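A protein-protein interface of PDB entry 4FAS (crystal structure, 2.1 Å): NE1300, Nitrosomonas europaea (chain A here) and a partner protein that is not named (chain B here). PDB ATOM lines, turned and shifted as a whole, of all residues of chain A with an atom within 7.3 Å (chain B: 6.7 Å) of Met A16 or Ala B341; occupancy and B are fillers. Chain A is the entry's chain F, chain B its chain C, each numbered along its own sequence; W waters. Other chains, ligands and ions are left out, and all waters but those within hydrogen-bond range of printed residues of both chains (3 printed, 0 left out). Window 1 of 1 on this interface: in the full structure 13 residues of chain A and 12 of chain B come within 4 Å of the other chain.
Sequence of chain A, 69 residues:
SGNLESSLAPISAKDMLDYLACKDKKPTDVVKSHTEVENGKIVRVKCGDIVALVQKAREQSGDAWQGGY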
ATOM      1  N   LEU A   8      13.821  20.461 -12.957  1.00  0.00           N
ATOM      2  CA  LEU A   8      12.833  21.367 -12.261  1.00  0.00           C
ATOM      3  C   LEU A   8      13.443  22.693 -11.687  1.00  0.00           C
ATOM      4  O   LEU A   8      14.583  22.711 -11.214  1.00  0.00           O
ATOM      5  CB  LEU A   8      12.122  20.622 -11.114  1.00  0.00           C
ATOM      6  CG  LEU A   8      11.108  19.506 -11.366  1.00  0.00           C
ATOM      7  CD1 LEU A   8      10.687  18.900 -10.059  1.00  0.00           C
ATOM      8  CD2 LEU A   8       9.894  20.000 -12.133  1.00  0.00           C
ATOM      9  N   ALA A   9      12.685  23.788 -11.712  1.00  0.00           N
ATOM     10  CA  ALA A   9      13.125  25.007 -11.046  1.00  0.00           C
ATOM     11  C   ALA A   9      13.308  24.688  -9.555  1.00  0.00           C
ATOM     12  O   ALA A   9      12.382  24.136  -8.956  1.00  0.00           O
ATOM     13  CB  ALA A   9      12.095  26.094 -11.219  1.00  0.00           C
ATOM     14  N   PRO A  10      14.490  25.010  -8.952  1.00  0.00           N
ATOM     15  CA  PRO A  10      14.681  24.832  -7.490  1.00  0.00           C
ATOM     16  C   PRO A  10      13.707  25.669  -6.636  1.00  0.00           C
ATOM     17  O   PRO A  10      13.596  26.852  -6.871  1.00  0.00           O
ATOM     18  CB  PRO A  10      16.122  25.326  -7.264  1.00  0.00           C
ATOM     19  CG  PRO A  10      16.785  25.112  -8.585  1.00  0.00           C
ATOM     20  CD  PRO A  10      15.735  25.468  -9.596  1.00  0.00           C
ATOM     21  N   ILE A  11      12.985  25.055  -5.696  1.00  0.00           N
ATOM     22  CA  ILE A  11      12.173  25.786  -4.743  1.00  0.00           C
ATOM     23  C   ILE A  11      12.724  25.410  -3.361  1.00  0.00           C
ATOM     24  O   ILE A  11      12.838  24.250  -3.045  1.00  0.00           O
ATOM     25  CB  ILE A  11      10.698  25.404  -4.816  1.00  0.00           C
ATOM     26  CG1 ILE A  11      10.200  25.451  -6.254  1.00  0.00           C
ATOM     27  CG2 ILE A  11       9.875  26.346  -3.988  1.00  0.00           C
ATOM     28  CD1 ILE A  11       8.703  25.116  -6.446  1.00  0.00           C
ATOM     29  N   SER A  12      13.073  26.382  -2.537  1.00  0.00           N
ATOM     30  CA  SER A  12      13.614  26.100  -1.212  1.00  0.00           C
ATOM     31  C   SER A  12      12.575  25.413  -0.358  1.00  0.00           C
ATOM     32  O   SER A  12      11.362  25.561  -0.586  1.00  0.00           O
ATOM     33  CB  SER A  12      13.995  27.390  -0.532  1.00  0.00           C
ATOM     34  OG  SER A  12      12.803  28.024  -0.115  1.00  0.00           O
ATOM     35  N   ALA A  13      13.056  24.691   0.647  1.00  0.00           N
ATOM     36  CA  ALA A  13      12.209  23.842   1.462  1.00  0.00           C
ATOM     37  C   ALA A  13      11.175  24.630   2.222  1.00  0.00           C
ATOM     38  O   ALA A  13      10.007  24.183   2.275  1.00  0.00           O
ATOM     39  CB  ALA A  13      13.018  22.959   2.432  1.00  0.00           C
ATOM     40  N   LYS A  14      11.590  25.779   2.797  1.00  0.00           N
ATOM     41  CA  LYS A  14      10.633  26.740   3.364  1.00  0.00           C
ATOM     42  C   LYS A  14       9.532  27.153   2.384  1.00  0.00           C
ATOM     43  O   LYS A  14       8.354  27.193   2.770  1.00  0.00           O
ATOM     44  CB  LYS A  14      11.291  27.914   4.066  1.00  0.00           C
ATOM     45  CG  LYS A  14      11.712  29.027   3.212  1.00  0.00           C
ATOM     46  CD  LYS A  14      12.182  30.140   4.108  1.00  0.00           C
ATOM     47  CE  LYS A  14      11.965  31.492   3.466  1.00  0.00           C
ATOM     48  NZ  LYS A  14      10.511  31.847   3.338  1.00  0.00           N
ATOM     49  N   ASP A  15       9.850  27.349   1.111  1.00  0.00           N
ATOM     50  CA  ASP A  15       8.759  27.721   0.172  1.00  0.00           C
ATOM     51  C   ASP A  15       7.793  26.595  -0.145  1.00  0.00           C
ATOM     52  O   ASP A  15       6.551  26.858  -0.244  1.00  0.00           O
ATOM     53  CB  ASP A  15       9.268  28.364  -1.114  1.00  0.00           C
ATOM     54  CG  ASP A  15      10.039  29.616  -0.840  1.00  0.00           C
ATOM     55  OD1 ASP A  15       9.602  30.385   0.015  1.00  0.00           O
ATOM     56  OD2 ASP A  15      11.097  29.828  -1.450  1.00  0.00           O
ATOM     57  N   MET A  16       8.350  25.371  -0.294  1.00  0.00           N
ATOM     58  CA  MET A  16       7.545  24.160  -0.452  1.00  0.00           C
ATOM     59  C   MET A  16       6.548  24.012   0.720  1.00  0.00           C
ATOM     60  O   MET A  16       5.376  23.643   0.560  1.00  0.00           O
ATOM     61  CB  MET A  16       8.427  22.913  -0.448  1.00  0.00           C
ATOM     62  CG  MET A  16       9.111  22.516  -1.715  1.00  0.00           C
ATOM     63  SD  MET A  16       8.144  22.566  -3.250  1.00  0.00           S
ATOM     64  CE  MET A  16       6.780  21.443  -3.035  1.00  0.00           C
ATOM     65  N   LEU A  17       7.053  24.247   1.919  1.00  0.00           N
ATOM     66  CA  LEU A  17       6.287  24.112   3.148  1.00  0.00           C
ATOM     67  C   LEU A  17       5.187  25.159   3.229  1.00  0.00           C
ATOM     68  O   LEU A  17       4.034  24.841   3.380  1.00  0.00           O
ATOM     69  CB  LEU A  17       7.256  24.305   4.294  1.00  0.00           C
ATOM     70  CG  LEU A  17       7.598  23.232   5.322  1.00  0.00           C
ATOM     71  CD1 LEU A  17       7.038  21.782   5.162  1.00  0.00           C
ATOM     72  CD2 LEU A  17       9.143  23.247   5.613  1.00  0.00           C
ATOM     73  N   ASP A  18       5.550  26.425   3.083  1.00  0.00           N
ATOM     74  CA  ASP A  18       4.534  27.466   2.909  1.00  0.00           C
ATOM     75  C   ASP A  18       3.506  27.105   1.819  1.00  0.00           C
ATOM     76  O   ASP A  18       2.290  27.252   2.063  1.00  0.00           O
ATOM     77  CB  ASP A  18       5.202  28.784   2.597  1.00  0.00           C
ATOM     78  CG  ASP A  18       6.079  29.276   3.762  1.00  0.00           C
ATOM     79  OD1 ASP A  18       5.884  28.743   4.896  1.00  0.00           O
ATOM     80  OD2 ASP A  18       6.988  30.145   3.532  1.00  0.00           O
ATOM     81  N   TYR A  19       3.962  26.642   0.643  1.00  0.00           N
ATOM     82  CA  TYR A  19       3.024  26.218  -0.411  1.00  0.00           C
ATOM     83  C   TYR A  19       2.065  25.167   0.111  1.00  0.00           C
ATOM     84  O   TYR A  19       0.865  25.242  -0.109  1.00  0.00           O
ATOM     85  CB  TYR A  19       3.777  25.638  -1.604  1.00  0.00           C
ATOM     86  CG  TYR A  19       2.904  25.231  -2.757  1.00  0.00           C
ATOM     87  CD1 TYR A  19       2.362  26.199  -3.627  1.00  0.00           C
ATOM     88  CD2 TYR A  19       2.639  23.885  -3.009  1.00  0.00           C
ATOM     89  CE1 TYR A  19       1.554  25.844  -4.695  1.00  0.00           C
ATOM     90  CE2 TYR A  19       1.842  23.497  -4.075  1.00  0.00           C
ATOM     91  CZ  TYR A  19       1.294  24.484  -4.916  1.00  0.00           C
ATOM     92  OH  TYR A  19       0.497  24.126  -5.976  1.00  0.00           O
ATOM     93  N   LEU A  20       2.591  24.172   0.819  1.00  0.00           N
ATOM     94  CA  LEU A  20       1.758  23.029   1.245  1.00  0.00           C
ATOM     95  C   LEU A  20       0.815  23.470   2.327  1.00  0.00           C
ATOM     96  O   LEU A  20      -0.307  22.977   2.393  1.00  0.00           O
ATOM     97  CB  LEU A  20       2.618  21.903   1.804  1.00  0.00           C
ATOM     98  CG  LEU A  20       3.364  20.985   0.870  1.00  0.00           C
ATOM     99  CD1 LEU A  20       4.284  20.155   1.768  1.00  0.00           C
ATOM    100  CD2 LEU A  20       2.370  20.128   0.060  1.00  0.00           C
ATOM    101  N   ALA A  21       1.293  24.383   3.187  1.00  0.00           N
ATOM    102  CA  ALA A  21       0.475  24.950   4.257  1.00  0.00           C
ATOM    103  C   ALA A  21      -0.722  25.727   3.694  1.00  0.00           C
ATOM    104  O   ALA A  21      -1.742  25.877   4.361  1.00  0.00           O
ATOM    105  CB  ALA A  21       1.301  25.850   5.170  1.00  0.00           C
ATOM    106  N   CYS A  22      -0.591  26.202   2.467  1.00  0.00           N
ATOM    107  CA  CYS A  22      -1.621  27.033   1.869  1.00  0.00           C
ATOM    108  C   CYS A  22      -2.564  26.231   0.977  1.00  0.00           C
ATOM    109  O   CYS A  22      -3.590  26.745   0.585  1.00  0.00           O
ATOM    110  CB  CYS A  22      -0.999  28.175   1.064  1.00  0.00           C
ATOM    111  SG  CYS A  22      -0.411  29.474   2.150  1.00  0.00           S
ATOM    112  N   LYS A  23      -2.240  24.965   0.702  1.00  0.00           N
ATOM    113  CA  LYS A  23      -2.927  24.244  -0.370  1.00  0.00           C
ATOM    114  C   LYS A  23      -4.460  24.181  -0.197  1.00  0.00           C
ATOM    115  O   LYS A  23      -5.201  24.281  -1.179  1.00  0.00           O
ATOM    116  CB  LYS A  23      -2.321  22.852  -0.606  1.00  0.00           C
ATOM    117  CG  LYS A  23      -2.011  22.576  -2.068  1.00  0.00           C
ATOM    118  CD  LYS A  23      -1.381  21.191  -2.160  1.00  0.00           C
ATOM    119  CE  LYS A  23      -0.214  21.104  -3.168  1.00  0.00           C
ATOM    120  NZ  LYS A  23      -0.625  21.334  -4.607  1.00  0.00           N
ATOM    121  N   ILE A  50       2.623  33.243  -1.746  1.00  0.00           N
ATOM    122  CA  ILE A  50       3.466  32.069  -1.837  1.00  0.00           C
ATOM    123  C   ILE A  50       3.062  31.203  -3.021  1.00  0.00           C
ATOM    124  O   ILE A  50       3.925  30.748  -3.756  1.00  0.00           O
ATOM    125  CB  ILE A  50       3.587  31.291  -0.495  1.00  0.00           C
ATOM    126  CG1 ILE A  50       4.946  30.561  -0.397  1.00  0.00           C
ATOM    127  CG2 ILE A  50       2.395  30.387  -0.211  1.00  0.00           C
ATOM    128  CD1 ILE A  50       5.275  29.469  -1.459  1.00  0.00           C
ATOM    129  N   LEU A  53       4.745  32.695  -5.809  1.00  0.00           N
ATOM    130  CA  LEU A  53       6.167  32.253  -5.838  1.00  0.00           C
ATOM    131  C   LEU A  53       6.386  30.822  -6.438  1.00  0.00           C
ATOM    132  O   LEU A  53       7.284  30.641  -7.262  1.00  0.00           O
ATOM    133  CB  LEU A  53       6.843  32.431  -4.452  1.00  0.00           C
ATOM    134  CG  LEU A  53       8.363  32.325  -4.241  1.00  0.00           C
ATOM    135  CD1 LEU A  53       8.865  33.160  -3.029  1.00  0.00           C
ATOM    136  CD2 LEU A  53       8.828  30.836  -4.144  1.00  0.00           C
ATOM    137  N   VAL A  54       5.572  29.825  -6.063  1.00  0.00           N
ATOM    138  CA  VAL A  54       5.672  28.492  -6.689  1.00  0.00           C
ATOM    139  C   VAL A  54       5.330  28.483  -8.189  1.00  0.00           C
ATOM    140  O   VAL A  54       6.218  28.209  -8.991  1.00  0.00           O
ATOM    141  CB  VAL A  54       4.933  27.386  -5.908  1.00  0.00           C
ATOM    142  CG1 VAL A  54       4.523  26.235  -6.831  1.00  0.00           C
ATOM    143  CG2 VAL A  54       5.828  26.873  -4.790  1.00  0.00           C
ATOM    144  N   GLN B 196      15.750  12.832 -11.540  1.00  0.00           N
ATOM    145  CA  GLN B 196      16.321  13.110 -10.208  1.00  0.00           C
ATOM    146  C   GLN B 196      17.460  12.155  -9.864  1.00  0.00           C
ATOM    147  O   GLN B 196      18.451  12.574  -9.299  1.00  0.00           O
ATOM    148  CB  GLN B 196      15.249  13.064  -9.120  1.00  0.00           C
ATOM    149  CG  GLN B 196      14.411  14.347  -9.024  1.00  0.00           C
ATOM    150  CD  GLN B 196      13.255  14.465 -10.015  1.00  0.00           C
ATOM    151  OE1 GLN B 196      13.071  13.657 -10.970  1.00  0.00           O
ATOM    152  NE2 GLN B 196      12.441  15.482  -9.773  1.00  0.00           N
ATOM    153  N   TRP B 331      10.726   9.806  -1.953  1.00  0.00           N
ATOM    154  CA  TRP B 331      11.795  10.543  -1.346  1.00  0.00           C
ATOM    155  C   TRP B 331      13.159   9.950  -1.608  1.00  0.00           C
ATOM    156  O   TRP B 331      14.122  10.689  -1.748  1.00  0.00           O
ATOM    157  CB  TRP B 331      11.549  10.570   0.144  1.00  0.00           C
ATOM    158  CG  TRP B 331      10.614  11.652   0.565  1.00  0.00           C
ATOM    159  CD1 TRP B 331       9.378  11.499   1.012  1.00  0.00           C
ATOM    160  CD2 TRP B 331      10.886  13.061   0.576  1.00  0.00           C
ATOM    161  NE1 TRP B 331       8.837  12.712   1.322  1.00  0.00           N
ATOM    162  CE2 TRP B 331       9.755  13.690   1.060  1.00  0.00           C
ATOM    163  CE3 TRP B 331      11.994  13.836   0.195  1.00  0.00           C
ATOM    164  CZ2 TRP B 331       9.656  15.073   1.184  1.00  0.00           C
ATOM    165  CZ3 TRP B 331      11.923  15.184   0.332  1.00  0.00           C
ATOM    166  CH2 TRP B 331      10.745  15.799   0.829  1.00  0.00           C
ATOM    167  N   PRO B 335      16.889  13.504   1.121  1.00  0.00           N
ATOM    168  CA  PRO B 335      15.877  14.559   0.799  1.00  0.00           C
ATOM    169  C   PRO B 335      16.417  15.783   0.019  1.00  0.00           C
ATOM    170  O   PRO B 335      15.600  16.525  -0.588  1.00  0.00           O
ATOM    171  CB  PRO B 335      15.382  15.011   2.169  1.00  0.00           C
ATOM    172  CG  PRO B 335      15.841  13.935   3.133  1.00  0.00           C
ATOM    173  CD  PRO B 335      17.012  13.217   2.558  1.00  0.00           C
ATOM    174  N   PHE B 336      17.755  15.987   0.045  1.00  0.00           N
ATOM    175  CA  PHE B 336      18.410  17.185  -0.488  1.00  0.00           C
ATOM    176  C   PHE B 336      18.810  16.943  -1.940  1.00  0.00           C
ATOM    177  O   PHE B 336      19.392  17.824  -2.538  1.00  0.00           O
ATOM    178  CB  PHE B 336      19.684  17.480   0.296  1.00  0.00           C
ATOM    179  CG  PHE B 336      20.608  16.281   0.376  1.00  0.00           C
ATOM    180  CD1 PHE B 336      21.385  15.908  -0.705  1.00  0.00           C
ATOM    181  CD2 PHE B 336      20.635  15.471   1.528  1.00  0.00           C
ATOM    182  CE1 PHE B 336      22.242  14.776  -0.644  1.00  0.00           C
ATOM    183  CE2 PHE B 336      21.399  14.374   1.584  1.00  0.00           C
ATOM    184  CZ  PHE B 336      22.245  14.012   0.492  1.00  0.00           C
ATOM    185  N   VAL B 337      18.537  15.769  -2.517  1.00  0.00           N
ATOM    186  CA  VAL B 337      18.895  15.539  -3.924  1.00  0.00           C
ATOM    187  C   VAL B 337      18.103  16.505  -4.790  1.00  0.00           C
ATOM    188  O   VAL B 337      16.892  16.591  -4.608  1.00  0.00           O
ATOM    189  CB  VAL B 337      18.576  14.081  -4.416  1.00  0.00           C
ATOM    190  CG1 VAL B 337      18.512  14.043  -5.954  1.00  0.00           C
ATOM    191  CG2 VAL B 337      19.583  13.057  -3.863  1.00  0.00           C
ATOM    192  N   PRO B 338      18.759  17.224  -5.730  1.00  0.00           N
ATOM    193  CA  PRO B 338      18.008  18.283  -6.461  1.00  0.00           C
ATOM    194  C   PRO B 338      16.821  17.765  -7.288  1.00  0.00           C
ATOM    195  O   PRO B 338      16.917  16.719  -7.958  1.00  0.00           O
ATOM    196  CB  PRO B 338      19.086  18.958  -7.329  1.00  0.00           C
ATOM    197  CG  PRO B 338      20.408  18.639  -6.590  1.00  0.00           C
ATOM    198  CD  PRO B 338      20.184  17.210  -6.131  1.00  0.00           C
ATOM    199  N   GLY B 339      15.697  18.487  -7.197  1.00  0.00           N
ATOM    200  CA  GLY B 339      14.424  18.046  -7.777  1.00  0.00           C
ATOM    201  C   GLY B 339      13.560  17.085  -6.948  1.00  0.00           C
ATOM    202  O   GLY B 339      12.349  16.909  -7.247  1.00  0.00           O
ATOM    203  N   ILE B 340      14.123  16.475  -5.896  1.00  0.00           N
ATOM    204  CA  ILE B 340      13.338  15.544  -5.096  1.00  0.00           C
ATOM    205  C   ILE B 340      12.220  16.246  -4.321  1.00  0.00           C
ATOM    206  O   ILE B 340      11.021  15.860  -4.432  1.00  0.00           O
ATOM    207  CB  ILE B 340      14.211  14.630  -4.158  1.00  0.00           C
ATOM    208  CG1 ILE B 340      15.006  13.592  -4.970  1.00  0.00           C
ATOM    209  CG2 ILE B 340      13.321  13.922  -3.156  1.00  0.00           C
ATOM    210  CD1 ILE B 340      14.198  12.772  -5.855  1.00  0.00           C
ATOM    211  N   ALA B 341      12.590  17.248  -3.526  1.00  0.00           N
ATOM    212  CA  ALA B 341      11.599  17.989  -2.745  1.00  0.00           C
ATOM    213  C   ALA B 341      10.564  18.728  -3.621  1.00  0.00           C
ATOM    214  O   ALA B 341       9.390  18.730  -3.321  1.00  0.00           O
ATOM    215  CB  ALA B 341      12.260  18.933  -1.804  1.00  0.00           C
ATOM    216  N   GLU B 342      11.029  19.335  -4.707  1.00  0.00           N
ATOM    217  CA  GLU B 342      10.155  20.011  -5.711  1.00  0.00           C
ATOM    218  C   GLU B 342       9.166  19.035  -6.358  1.00  0.00           C
ATOM    219  O   GLU B 342       8.072  19.446  -6.830  1.00  0.00           O
ATOM    220  CB  GLU B 342      11.019  20.612  -6.810  1.00  0.00           C
ATOM    221  CG  GLU B 342      11.918  21.721  -6.278  1.00  0.00           C
ATOM    222  CD  GLU B 342      13.337  21.272  -5.820  1.00  0.00           C
ATOM    223  OE1 GLU B 342      13.624  20.074  -5.612  1.00  0.00           O
ATOM    224  OE2 GLU B 342      14.168  22.173  -5.648  1.00  0.00           O
ATOM    225  N   ASN B 343       9.553  17.744  -6.382  1.00  0.00           N
ATOM    226  CA  ASN B 343       8.769  16.720  -7.074  1.00  0.00           C
ATOM    227  C   ASN B 343       7.686  16.215  -6.121  1.00  0.00           C
ATOM    228  O   ASN B 343       6.776  15.647  -6.583  1.00  0.00           O
ATOM    229  CB  ASN B 343       9.678  15.627  -7.677  1.00  0.00           C
ATOM    230  CG  ASN B 343       8.900  14.445  -8.317  1.00  0.00           C
ATOM    231  OD1 ASN B 343       8.083  14.633  -9.261  1.00  0.00           O
ATOM    232  ND2 ASN B 343       9.148  13.207  -7.800  1.00  0.00           N
ATOM    233  N   ILE B 344       7.754  16.528  -4.808  1.00  0.00           N
ATOM    234  CA  ILE B 344       6.931  15.837  -3.805  1.00  0.00           C
ATOM    235  C   ILE B 344       5.424  16.017  -3.974  1.00  0.00           C
ATOM    236  O   ILE B 344       4.651  15.179  -3.519  1.00  0.00           O
ATOM    237  CB  ILE B 344       7.385  16.064  -2.330  1.00  0.00           C
ATOM    238  CG1 ILE B 344       7.115  14.781  -1.514  1.00  0.00           C
ATOM    239  CG2 ILE B 344       6.707  17.252  -1.678  1.00  0.00           C
ATOM    240  CD1 ILE B 344       8.007  13.657  -1.901  1.00  0.00           C
ATOM    241  N   THR B 345       5.017  17.102  -4.632  1.00  0.00           N
ATOM    242  CA  THR B 345       3.603  17.408  -4.884  1.00  0.00           C
ATOM    243  C   THR B 345       3.164  17.072  -6.316  1.00  0.00           C
ATOM    244  O   THR B 345       2.025  17.279  -6.673  1.00  0.00           O
ATOM    245  CB  THR B 345       3.343  18.906  -4.749  1.00  0.00           C
ATOM    246  OG1 THR B 345       4.312  19.580  -5.554  1.00  0.00           O
ATOM    247  CG2 THR B 345       3.536  19.399  -3.306  1.00  0.00           C
ATOM    248  N   LEU B 381      10.738  17.983   4.991  1.00  0.00           N
ATOM    249  CA  LEU B 381      10.993  19.305   4.446  1.00  0.00           C
ATOM    250  C   LEU B 381      11.452  20.275   5.534  1.00  0.00           C
ATOM    251  O   LEU B 381      12.294  21.157   5.261  1.00  0.00           O
ATOM    252  CB  LEU B 381       9.695  19.818   3.744  1.00  0.00           C
ATOM    253  CG  LEU B 381       9.251  19.313   2.383  1.00  0.00           C
ATOM    254  CD1 LEU B 381       7.851  19.761   1.950  1.00  0.00           C
ATOM    255  CD2 LEU B 381      10.268  19.632   1.298  1.00  0.00           C
ATOM    256  N   LEU B 384      15.014  19.529   5.812  1.00  0.00           N
ATOM    257  CA  LEU B 384      15.687  20.046   4.602  1.00  0.00           C
ATOM    258  C   LEU B 384      15.957  21.552   4.708  1.00  0.00           C
ATOM    259  O   LEU B 384      17.097  22.006   4.446  1.00  0.00           O
ATOM    260  CB  LEU B 384      14.883  19.697   3.345  1.00  0.00           C
ATOM    261  CG  LEU B 384      15.511  20.145   2.033  1.00  0.00           C
ATOM    262  CD1 LEU B 384      16.948  19.565   1.910  1.00  0.00           C
ATOM    263  CD2 LEU B 384      14.605  19.759   0.887  1.00  0.00           C
ATOM    264  N   GLN B 388      19.373  23.551   4.645  1.00  0.00           N
ATOM    265  CA  GLN B 388      19.577  24.562   3.585  1.00  0.00           C
ATOM    266  C   GLN B 388      20.106  25.904   4.115  1.00  0.00           C
ATOM    267  O   GLN B 388      21.024  26.438   3.548  1.00  0.00           O
ATOM    268  CB  GLN B 388      18.344  24.738   2.715  1.00  0.00           C
ATOM    269  CG  GLN B 388      18.213  23.702   1.668  1.00  0.00           C
ATOM    270  CD  GLN B 388      16.890  23.824   0.972  1.00  0.00           C
ATOM    271  OE1 GLN B 388      15.984  24.561   1.430  1.00  0.00           O
ATOM    272  NE2 GLN B 388      16.732  23.092  -0.120  1.00  0.00           N
HETATM  273  O   HOH W   1      14.400  22.463  -1.734  1.00  0.00           O
HETATM  274  O   HOH W   2      14.502  26.163   2.659  1.00  0.00           O
HETATM  275  O   HOH W   3      15.424  21.023  -9.499  1.00  0.00           O
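Gly B339 touches Leu A8. Glu B342 touches Leu A8 (CB to CD1, 3.7 Å). Glu B342 touches Ala A9. CA of Pro A10 touches OE2 of Glu B342, 3.3 Å away. CA of Ser A12 touches OE1 of Gln B388 (3.9 Å). Leu B381 touches Ala A13 (O to CB, 3.4 Å). Leu B384 touches Ala A13 (CG to CB, 3.8 Å). O of Ala B341 touches CE of Met A16, 3.8 Å away. Met A16 touches Thr B345 (CE to CG2, 3.8 Å). Leu A20 touches Leu B381 (CD1 to CD1, 3.6 Å).
Of the 16 printed residues of chain B, 8 touch a printed residue of chain A. Printed residues of chain B that touch a printed residue of chain A: Gln B196, Gly B339, Ala B341, Glu B342, Thr B345, Leu B381, Leu B384 and Gln B388. Among the printed residues, no Asp or Glu carboxylate lies within 4 Å of a Lys or Arg side-chain nitrogen of the other chain.
OE2 of Glu B342 sits at hydrogen-bond distance from N of Ile A11 (3.1 Å). The side-chain amide oxygen of Gln B388 is in hydrogen-bond range of the backbone NH of Ala A13.
Water W2 lies within hydrogen-bond range of the side-chain amide oxygen (OE1) of Gln B388 (2.5 Å), the backbone NH (N) of Ala A13 (2.9 Å) and the backbone NH (N) of Lys A14 (2.9 Å). Water W3 bridges the backbone carbonyl oxygen (O) of Leu A8 (2.5 Å) and the backbone NH (N) of Gly B339 (3.4 Å). Water W1 lies within hydrogen-bond range of O of Ile A11 (2.7 Å) and NE2 of Gln B388 (2.9 Å).
The backbone carbonyl oxygen (O) of Gly B339 lies within hydrogen-bond range of the side-chain amide nitrogen (NE2) of Gln B196 (2.9 Å). OE1 of Glu B342 is in hydrogen-bond range of N of Gly B339, at 3.1 Å. OG of Ser A12 lies within hydrogen-bond range of OD2 of Asp A15, 2.8 Å away.
Of the printed residues of chain B, Leu A20 touches Thr B345 (3.6 Å) and Leu B381 (3.6 Å). Of the printed residues of chain A, Ala B341 touches Met A16. Printed residues of chain A within 4 Å of Glu B342: Leu A8 (3.7 Å), Ala A9 (3.6 Å), Pro A10 (3.3 Å) and Ile A11 (3.1 Å). The nearest printed residue of chain B that does not touch Met A16 is Leu B381 (4.002 Å).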
